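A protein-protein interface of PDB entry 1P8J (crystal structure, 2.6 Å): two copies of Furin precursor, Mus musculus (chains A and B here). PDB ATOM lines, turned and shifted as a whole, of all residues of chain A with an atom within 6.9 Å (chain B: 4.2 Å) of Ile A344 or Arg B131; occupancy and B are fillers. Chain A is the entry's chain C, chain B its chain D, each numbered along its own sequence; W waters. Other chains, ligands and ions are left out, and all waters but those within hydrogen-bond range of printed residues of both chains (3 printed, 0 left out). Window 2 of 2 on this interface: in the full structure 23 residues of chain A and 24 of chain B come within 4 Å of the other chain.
Water W2 bridges O of Gly B134 (2.7 Å) and ND2 of Asn A372 (2.9 Å).
Water W1 lies within hydrogen-bond range of the side-chain amino group of Lys A342 (2.7 Å) and the backbone carbonyl oxygen of Leu B162 (2.9 Å).
Water W3 lies within hydrogen-bond range of O of Val B68 and OE2 of Glu A346.
Among the printed residues, pairs that only touch across the chains: Glu A346 with Ala B127, Ile A344 with Arg B131, Ile A344 with Ala B130 and Glu A346 with Val B128.
The backbone carbonyl oxygen (O) of Val B128 is in hydrogen-bond range of the side-chain hydroxyl (OG) of Ser B132 (2.8 Å).
The side-chain sulfur (SG) of Cys A367 forms a disulfide with the side-chain sulfur (SG) of Cys A343, 2.1 Å away.
OE1 of Gln B71 sits at hydrogen-bond distance from NH1 of Arg B131 (2.8 Å).
Printed residues of chain B within 4 Å of Ile A344: Ala B130 and Arg B131.
Arg B131 touches just these residues of chain A: Ile A344 (3.7 Å) and Glu A370 (3.7 Å).
Printed residues of chain A within 4 Å of Val B128: Glu A346.
Printed residues of chain A within 4 Å of Ala B127: Glu A346 (3.5 Å).
Of the printed residues of chain B, Glu A346 touches Ala B127 and Val B128.
Of the printed residues of chain A, Ala B130 touches Ile A344 (3.8 Å).
Printed residues of chain B within 4 Å of Glu A370: Arg B131.
Leu B162 touches none of the printed residues of chain A.
The nearest residue of chain B that does not touch Ile A344 is Ala B127 (4.1 Å).
The nearest residue of chain A that does not touch Arg B131 is Glu A346 (4.6 Å).
The nearest printed residue of chain B that does not touch Glu A370 is Gln B71 (4.3 Å).
The side-chain carboxylate (OE1) of Glu A370 is in salt-bridge range of the guanidinium group (NH1) of Arg B131 (3.7 Å).
Of the 12 printed residues of chain B, 4 touch a printed residue of chain A.
Hydrophobic or aromatic side chains of chain B within 4 Å of the printed part of chain A: Ala B127, Val B128 and Ala B130.
Of the 12 printed residues of chain A, 3 touch a printed residue of chain B.
Among the printed residues, 5 pairs touch across the chains.
Among the printed residues, Asp or Glu carboxylates within 4 Å of a Lys or Arg side-chain nitrogen of the other chain: Glu A370 with Arg B131 (3.7 Å).
No position is printed for both chains.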
ATOM      1  N   LYS A 342     -29.538  -6.599 -18.400  1.00  0.00           N
ATOM      2  CA  LYS A 342     -28.185  -6.302 -18.861  1.00  0.00           C
ATOM      3  C   LYS A 342     -28.041  -6.842 -20.263  1.00  0.00           C
ATOM      4  O   LYS A 342     -28.015  -8.047 -20.467  1.00  0.00           O
ATOM      5  CB  LYS A 342     -27.161  -6.970 -17.947  1.00  0.00           C
ATOM      6  CG  LYS A 342     -25.716  -6.668 -18.289  1.00  0.00           C
ATOM      7  CD  LYS A 342     -24.796  -7.415 -17.345  1.00  0.00           C
ATOM      8  CE  LYS A 342     -23.348  -7.075 -17.589  1.00  0.00           C
ATOM      9  NZ  LYS A 342     -22.476  -7.677 -16.547  1.00  0.00           N
ATOM     10  N   CYS A 343     -27.954  -5.957 -21.239  1.00  0.00           N
ATOM     11  CA  CYS A 343     -27.831  -6.407 -22.608  1.00  0.00           C
ATOM     12  C   CYS A 343     -26.424  -6.138 -23.124  1.00  0.00           C
ATOM     13  O   CYS A 343     -25.986  -4.991 -23.193  1.00  0.00           O
ATOM     14  CB  CYS A 343     -28.877  -5.710 -23.482  1.00  0.00           C
ATOM     15  SG  CYS A 343     -28.848  -6.254 -25.215  1.00  0.00           S
ATOM     16  N   ILE A 344     -25.721  -7.215 -23.466  1.00  0.00           N
ATOM     17  CA  ILE A 344     -24.358  -7.146 -23.975  1.00  0.00           C
ATOM     18  C   ILE A 344     -24.382  -7.283 -25.481  1.00  0.00           C
ATOM     19  O   ILE A 344     -24.915  -8.254 -25.994  1.00  0.00           O
ATOM     20  CB  ILE A 344     -23.507  -8.309 -23.434  1.00  0.00           C
ATOM     21  CG1 ILE A 344     -23.449  -8.251 -21.911  1.00  0.00           C
ATOM     22  CG2 ILE A 344     -22.115  -8.268 -24.033  1.00  0.00           C
ATOM     23  CD1 ILE A 344     -22.788  -9.460 -21.285  1.00  0.00           C
ATOM     24  N   VAL A 345     -23.809  -6.321 -26.191  1.00  0.00           N
ATOM     25  CA  VAL A 345     -23.770  -6.400 -27.641  1.00  0.00           C
ATOM     26  C   VAL A 345     -22.383  -6.073 -28.208  1.00  0.00           C
ATOM     27  O   VAL A 345     -21.835  -4.991 -27.985  1.00  0.00           O
ATOM     28  CB  VAL A 345     -24.865  -5.495 -28.283  1.00  0.00           C
ATOM     29  CG1 VAL A 345     -25.140  -4.314 -27.407  1.00  0.00           C
ATOM     30  CG2 VAL A 345     -24.442  -5.034 -29.667  1.00  0.00           C
ATOM     31  N   GLU A 346     -21.817  -7.041 -28.927  1.00  0.00           N
ATOM     32  CA  GLU A 346     -20.506  -6.908 -29.551  1.00  0.00           C
ATOM     33  C   GLU A 346     -20.685  -6.097 -30.824  1.00  0.00           C
ATOM     34  O   GLU A 346     -21.330  -6.556 -31.761  1.00  0.00           O
ATOM     35  CB  GLU A 346     -19.956  -8.299 -29.880  1.00  0.00           C
ATOM     36  CG  GLU A 346     -19.898  -9.226 -28.671  1.00  0.00           C
ATOM     37  CD  GLU A 346     -19.569 -10.670 -29.030  1.00  0.00           C
ATOM     38  OE1 GLU A 346     -18.369 -11.007 -29.213  1.00  0.00           O
ATOM     39  OE2 GLU A 346     -20.529 -11.470 -29.135  1.00  0.00           O
ATOM     40  N   CYS A 367     -31.340  -6.534 -27.417  1.00  0.00           N
ATOM     41  CA  CYS A 367     -31.792  -7.843 -26.953  1.00  0.00           C
ATOM     42  C   CYS A 367     -33.291  -8.096 -27.148  1.00  0.00           C
ATOM     43  O   CYS A 367     -33.946  -8.726 -26.312  1.00  0.00           O
ATOM     44  CB  CYS A 367     -31.408  -8.018 -25.472  1.00  0.00           C
ATOM     45  SG  CYS A 367     -29.604  -8.169 -25.171  1.00  0.00           S
ATOM     46  N   GLU A 370     -35.386 -11.328 -26.220  1.00  0.00           N
ATOM     47  CA  GLU A 370     -34.625 -12.045 -25.204  1.00  0.00           C
ATOM     48  C   GLU A 370     -35.005 -11.520 -23.824  1.00  0.00           C
ATOM     49  O   GLU A 370     -35.587 -10.445 -23.695  1.00  0.00           O
ATOM     50  CB  GLU A 370     -33.124 -11.852 -25.433  1.00  0.00           C
ATOM     51  CG  GLU A 370     -32.675 -12.135 -26.864  1.00  0.00           C
ATOM     52  CD  GLU A 370     -31.184 -11.898 -27.064  1.00  0.00           C
ATOM     53  OE1 GLU A 370     -30.721 -11.960 -28.230  1.00  0.00           O
ATOM     54  OE2 GLU A 370     -30.476 -11.654 -26.055  1.00  0.00           O
ATOM     55  N   ASN A 372     -33.293 -10.146 -21.622  1.00  0.00           N
ATOM     56  CA  ASN A 372     -32.629  -8.890 -21.293  1.00  0.00           C
ATOM     57  C   ASN A 372     -33.016  -7.728 -22.190  1.00  0.00           C
ATOM     58  O   ASN A 372     -32.336  -6.698 -22.220  1.00  0.00           O
ATOM     59  CB  ASN A 372     -31.103  -9.065 -21.309  1.00  0.00           C
ATOM     60  CG  ASN A 372     -30.585  -9.752 -20.063  1.00  0.00           C
ATOM     61  OD1 ASN A 372     -30.674  -9.206 -18.958  1.00  0.00           O
ATOM     62  ND2 ASN A 372     -30.045 -10.956 -20.230  1.00  0.00           N
ATOM     63  N   THR A 460     -17.534  -3.219 -27.192  1.00  0.00           N
ATOM     64  CA  THR A 460     -18.691  -3.907 -26.662  1.00  0.00           C
ATOM     65  C   THR A 460     -19.588  -2.883 -25.988  1.00  0.00           C
ATOM     66  O   THR A 460     -19.155  -2.119 -25.118  1.00  0.00           O
ATOM     67  CB  THR A 460     -18.288  -4.977 -25.644  1.00  0.00           C
ATOM     68  OG1 THR A 460     -17.475  -5.961 -26.291  1.00  0.00           O
ATOM     69  CG2 THR A 460     -19.516  -5.665 -25.079  1.00  0.00           C
ATOM     70  N   LEU A 461     -20.838  -2.845 -26.422  1.00  0.00           N
ATOM     71  CA  LEU A 461     -21.807  -1.927 -25.845  1.00  0.00           C
ATOM     72  C   LEU A 461     -22.596  -2.714 -24.811  1.00  0.00           C
ATOM     73  O   LEU A 461     -23.194  -3.742 -25.135  1.00  0.00           O
ATOM     74  CB  LEU A 461     -22.750  -1.417 -26.928  1.00  0.00           C
ATOM     75  CG  LEU A 461     -23.798  -0.378 -26.535  1.00  0.00           C
ATOM     76  CD1 LEU A 461     -23.123   0.919 -26.160  1.00  0.00           C
ATOM     77  CD2 LEU A 461     -24.732  -0.157 -27.719  1.00  0.00           C
ATOM     78  N   VAL A 462     -22.566  -2.267 -23.563  1.00  0.00           N
ATOM     79  CA  VAL A 462     -23.324  -2.948 -22.524  1.00  0.00           C
ATOM     80  C   VAL A 462     -24.419  -2.008 -22.060  1.00  0.00           C
ATOM     81  O   VAL A 462     -24.158  -0.892 -21.565  1.00  0.00           O
ATOM     82  CB  VAL A 462     -22.459  -3.337 -21.327  1.00  0.00           C
ATOM     83  CG1 VAL A 462     -23.317  -3.998 -20.283  1.00  0.00           C
ATOM     84  CG2 VAL A 462     -21.361  -4.279 -21.777  1.00  0.00           C
ATOM     85  N   LEU A 463     -25.652  -2.460 -22.244  1.00  0.00           N
ATOM     86  CA  LEU A 463     -26.817  -1.675 -21.876  1.00  0.00           C
ATOM     87  C   LEU A 463     -27.480  -2.184 -20.599  1.00  0.00           C
ATOM     88  O   LEU A 463     -27.775  -3.370 -20.473  1.00  0.00           O
ATOM     89  CB  LEU A 463     -27.836  -1.723 -23.012  1.00  0.00           C
ATOM     90  CG  LEU A 463     -27.305  -1.415 -24.403  1.00  0.00           C
ATOM     91  CD1 LEU A 463     -28.431  -1.546 -25.386  1.00  0.00           C
ATOM     92  CD2 LEU A 463     -26.726  -0.016 -24.445  1.00  0.00           C
ATOM     93  N   VAL B  68     -24.773 -18.269 -29.827  1.00  0.00           N
ATOM     94  CA  VAL B  68     -24.054 -17.029 -29.586  1.00  0.00           C
ATOM     95  C   VAL B  68     -22.985 -16.786 -30.649  1.00  0.00           C
ATOM     96  O   VAL B  68     -22.658 -15.641 -30.955  1.00  0.00           O
ATOM     97  CB  VAL B  68     -23.396 -17.050 -28.192  1.00  0.00           C
ATOM     98  CG1 VAL B  68     -22.662 -15.741 -27.950  1.00  0.00           C
ATOM     99  CG2 VAL B  68     -24.462 -17.276 -27.117  1.00  0.00           C
ATOM    100  N   GLN B  71     -25.105 -15.405 -33.378  1.00  0.00           N
ATOM    101  CA  GLN B  71     -26.135 -14.467 -32.963  1.00  0.00           C
ATOM    102  C   GLN B  71     -27.480 -14.859 -33.567  1.00  0.00           C
ATOM    103  O   GLN B  71     -28.111 -14.080 -34.290  1.00  0.00           O
ATOM    104  CB  GLN B  71     -25.760 -13.047 -33.395  1.00  0.00           C
ATOM    105  CG  GLN B  71     -25.675 -12.080 -32.228  1.00  0.00           C
ATOM    106  CD  GLN B  71     -26.985 -11.991 -31.442  1.00  0.00           C
ATOM    107  OE1 GLN B  71     -27.016 -11.487 -30.314  1.00  0.00           O
ATOM    108  NE2 GLN B  71     -28.073 -12.475 -32.040  1.00  0.00           N
ATOM    109  N   ALA B 127     -17.249 -11.574 -24.139  1.00  0.00           N
ATOM    110  CA  ALA B 127     -18.663 -11.292 -24.358  1.00  0.00           C
ATOM    111  C   ALA B 127     -19.451 -12.557 -24.676  1.00  0.00           C
ATOM    112  O   ALA B 127     -20.606 -12.697 -24.254  1.00  0.00           O
ATOM    113  CB  ALA B 127     -18.836 -10.286 -25.481  1.00  0.00           C
ATOM    114  N   VAL B 128     -18.838 -13.473 -25.420  1.00  0.00           N
ATOM    115  CA  VAL B 128     -19.501 -14.718 -25.768  1.00  0.00           C
ATOM    116  C   VAL B 128     -19.730 -15.570 -24.528  1.00  0.00           C
ATOM    117  O   VAL B 128     -20.819 -16.126 -24.340  1.00  0.00           O
ATOM    118  CB  VAL B 128     -18.682 -15.518 -26.786  1.00  0.00           C
ATOM    119  CG1 VAL B 128     -19.222 -16.942 -26.915  1.00  0.00           C
ATOM    120  CG2 VAL B 128     -18.746 -14.829 -28.123  1.00  0.00           C
ATOM    121  N   GLU B 129     -18.719 -15.682 -23.676  1.00  0.00           N
ATOM    122  CA  GLU B 129     -18.886 -16.474 -22.466  1.00  0.00           C
ATOM    123  C   GLU B 129     -19.952 -15.829 -21.566  1.00  0.00           C
ATOM    124  O   GLU B 129     -20.827 -16.511 -21.043  1.00  0.00           O
ATOM    125  CB  GLU B 129     -17.556 -16.585 -21.717  1.00  0.00           C
ATOM    126  CG  GLU B 129     -16.398 -17.111 -22.557  1.00  0.00           C
ATOM    127  CD  GLU B 129     -15.207 -17.504 -21.696  1.00  0.00           C
ATOM    128  OE1 GLU B 129     -15.057 -16.911 -20.606  1.00  0.00           O
ATOM    129  OE2 GLU B 129     -14.423 -18.393 -22.102  1.00  0.00           O
ATOM    130  N   ALA B 130     -19.877 -14.509 -21.404  1.00  0.00           N
ATOM    131  CA  ALA B 130     -20.819 -13.782 -20.562  1.00  0.00           C
ATOM    132  C   ALA B 130     -22.265 -13.953 -21.029  1.00  0.00           C
ATOM    133  O   ALA B 130     -23.173 -14.112 -20.216  1.00  0.00           O
ATOM    134  CB  ALA B 130     -20.453 -12.309 -20.524  1.00  0.00           C
ATOM    135  N   ARG B 131     -22.488 -13.915 -22.336  1.00  0.00           N
ATOM    136  CA  ARG B 131     -23.840 -14.082 -22.855  1.00  0.00           C
ATOM    137  C   ARG B 131     -24.311 -15.521 -22.684  1.00  0.00           C
ATOM    138  O   ARG B 131     -25.500 -15.774 -22.487  1.00  0.00           O
ATOM    139  CB  ARG B 131     -23.912 -13.692 -24.328  1.00  0.00           C
ATOM    140  CG  ARG B 131     -23.572 -12.244 -24.577  1.00  0.00           C
ATOM    141  CD  ARG B 131     -23.842 -11.878 -26.026  1.00  0.00           C
ATOM    142  NE  ARG B 131     -25.274 -11.894 -26.305  1.00  0.00           N
ATOM    143  CZ  ARG B 131     -25.812 -12.306 -27.451  1.00  0.00           C
ATOM    144  NH1 ARG B 131     -27.135 -12.283 -27.610  1.00  0.00           N
ATOM    145  NH2 ARG B 131     -25.031 -12.755 -28.434  1.00  0.00           N
ATOM    146  N   SER B 132     -23.379 -16.465 -22.751  1.00  0.00           N
ATOM    147  CA  SER B 132     -23.731 -17.865 -22.586  1.00  0.00           C
ATOM    148  C   SER B 132     -24.051 -18.173 -21.128  1.00  0.00           C
ATOM    149  O   SER B 132     -25.092 -18.749 -20.821  1.00  0.00           O
ATOM    150  CB  SER B 132     -22.591 -18.743 -23.087  1.00  0.00           C
ATOM    151  OG  SER B 132     -22.361 -18.482 -24.463  1.00  0.00           O
ATOM    152  N   LEU B 133     -23.166 -17.776 -20.225  1.00  0.00           N
ATOM    153  CA  LEU B 133     -23.379 -18.020 -18.808  1.00  0.00           C
ATOM    154  C   LEU B 133     -24.621 -17.287 -18.290  1.00  0.00           C
ATOM    155  O   LEU B 133     -25.269 -17.731 -17.333  1.00  0.00           O
ATOM    156  CB  LEU B 133     -22.153 -17.566 -18.025  1.00  0.00           C
ATOM    157  CG  LEU B 133     -20.861 -18.318 -18.332  1.00  0.00           C
ATOM    158  CD1 LEU B 133     -19.686 -17.599 -17.666  1.00  0.00           C
ATOM    159  CD2 LEU B 133     -20.988 -19.742 -17.825  1.00  0.00           C
ATOM    160  N   GLY B 134     -24.954 -16.167 -18.927  1.00  0.00           N
ATOM    161  CA  GLY B 134     -26.101 -15.395 -18.494  1.00  0.00           C
ATOM    162  C   GLY B 134     -27.358 -15.540 -19.333  1.00  0.00           C
ATOM    163  O   GLY B 134     -28.238 -14.674 -19.277  1.00  0.00           O
ATOM    164  N   LEU B 135     -27.458 -16.622 -20.098  1.00  0.00           N
ATOM    165  CA  LEU B 135     -28.632 -16.861 -20.937  1.00  0.00           C
ATOM    166  C   LEU B 135     -29.840 -17.343 -20.136  1.00  0.00           C
ATOM    167  O   LEU B 135     -29.772 -18.389 -19.494  1.00  0.00           O
ATOM    168  CB  LEU B 135     -28.315 -17.917 -21.995  1.00  0.00           C
ATOM    169  CG  LEU B 135     -29.467 -18.324 -22.922  1.00  0.00           C
ATOM    170  CD1 LEU B 135     -29.579 -17.320 -24.070  1.00  0.00           C
ATOM    171  CD2 LEU B 135     -29.214 -19.716 -23.475  1.00  0.00           C
ATOM    172  N   LEU B 162     -16.284  -9.472 -18.200  1.00  0.00           N
ATOM    173  CA  LEU B 162     -17.708  -9.717 -18.364  1.00  0.00           C
ATOM    174  C   LEU B 162     -18.141 -11.103 -17.920  1.00  0.00           C
ATOM    175  O   LEU B 162     -19.234 -11.277 -17.385  1.00  0.00           O
ATOM    176  CB  LEU B 162     -18.132  -9.485 -19.807  1.00  0.00           C
ATOM    177  CG  LEU B 162     -18.189  -8.028 -20.284  1.00  0.00           C
ATOM    178  CD1 LEU B 162     -18.664  -8.002 -21.724  1.00  0.00           C
ATOM    179  CD2 LEU B 162     -19.126  -7.210 -19.406  1.00  0.00           C
HETATM  180  O   HOH W   1     -21.889 -10.084 -17.699  1.00  0.00           O
HETATM  181  O   HOH W   2     -28.478 -12.273 -18.132  1.00  0.00           O
HETATM  182  O   HOH W   3     -20.208 -13.646 -31.560  1.00  0.00           O
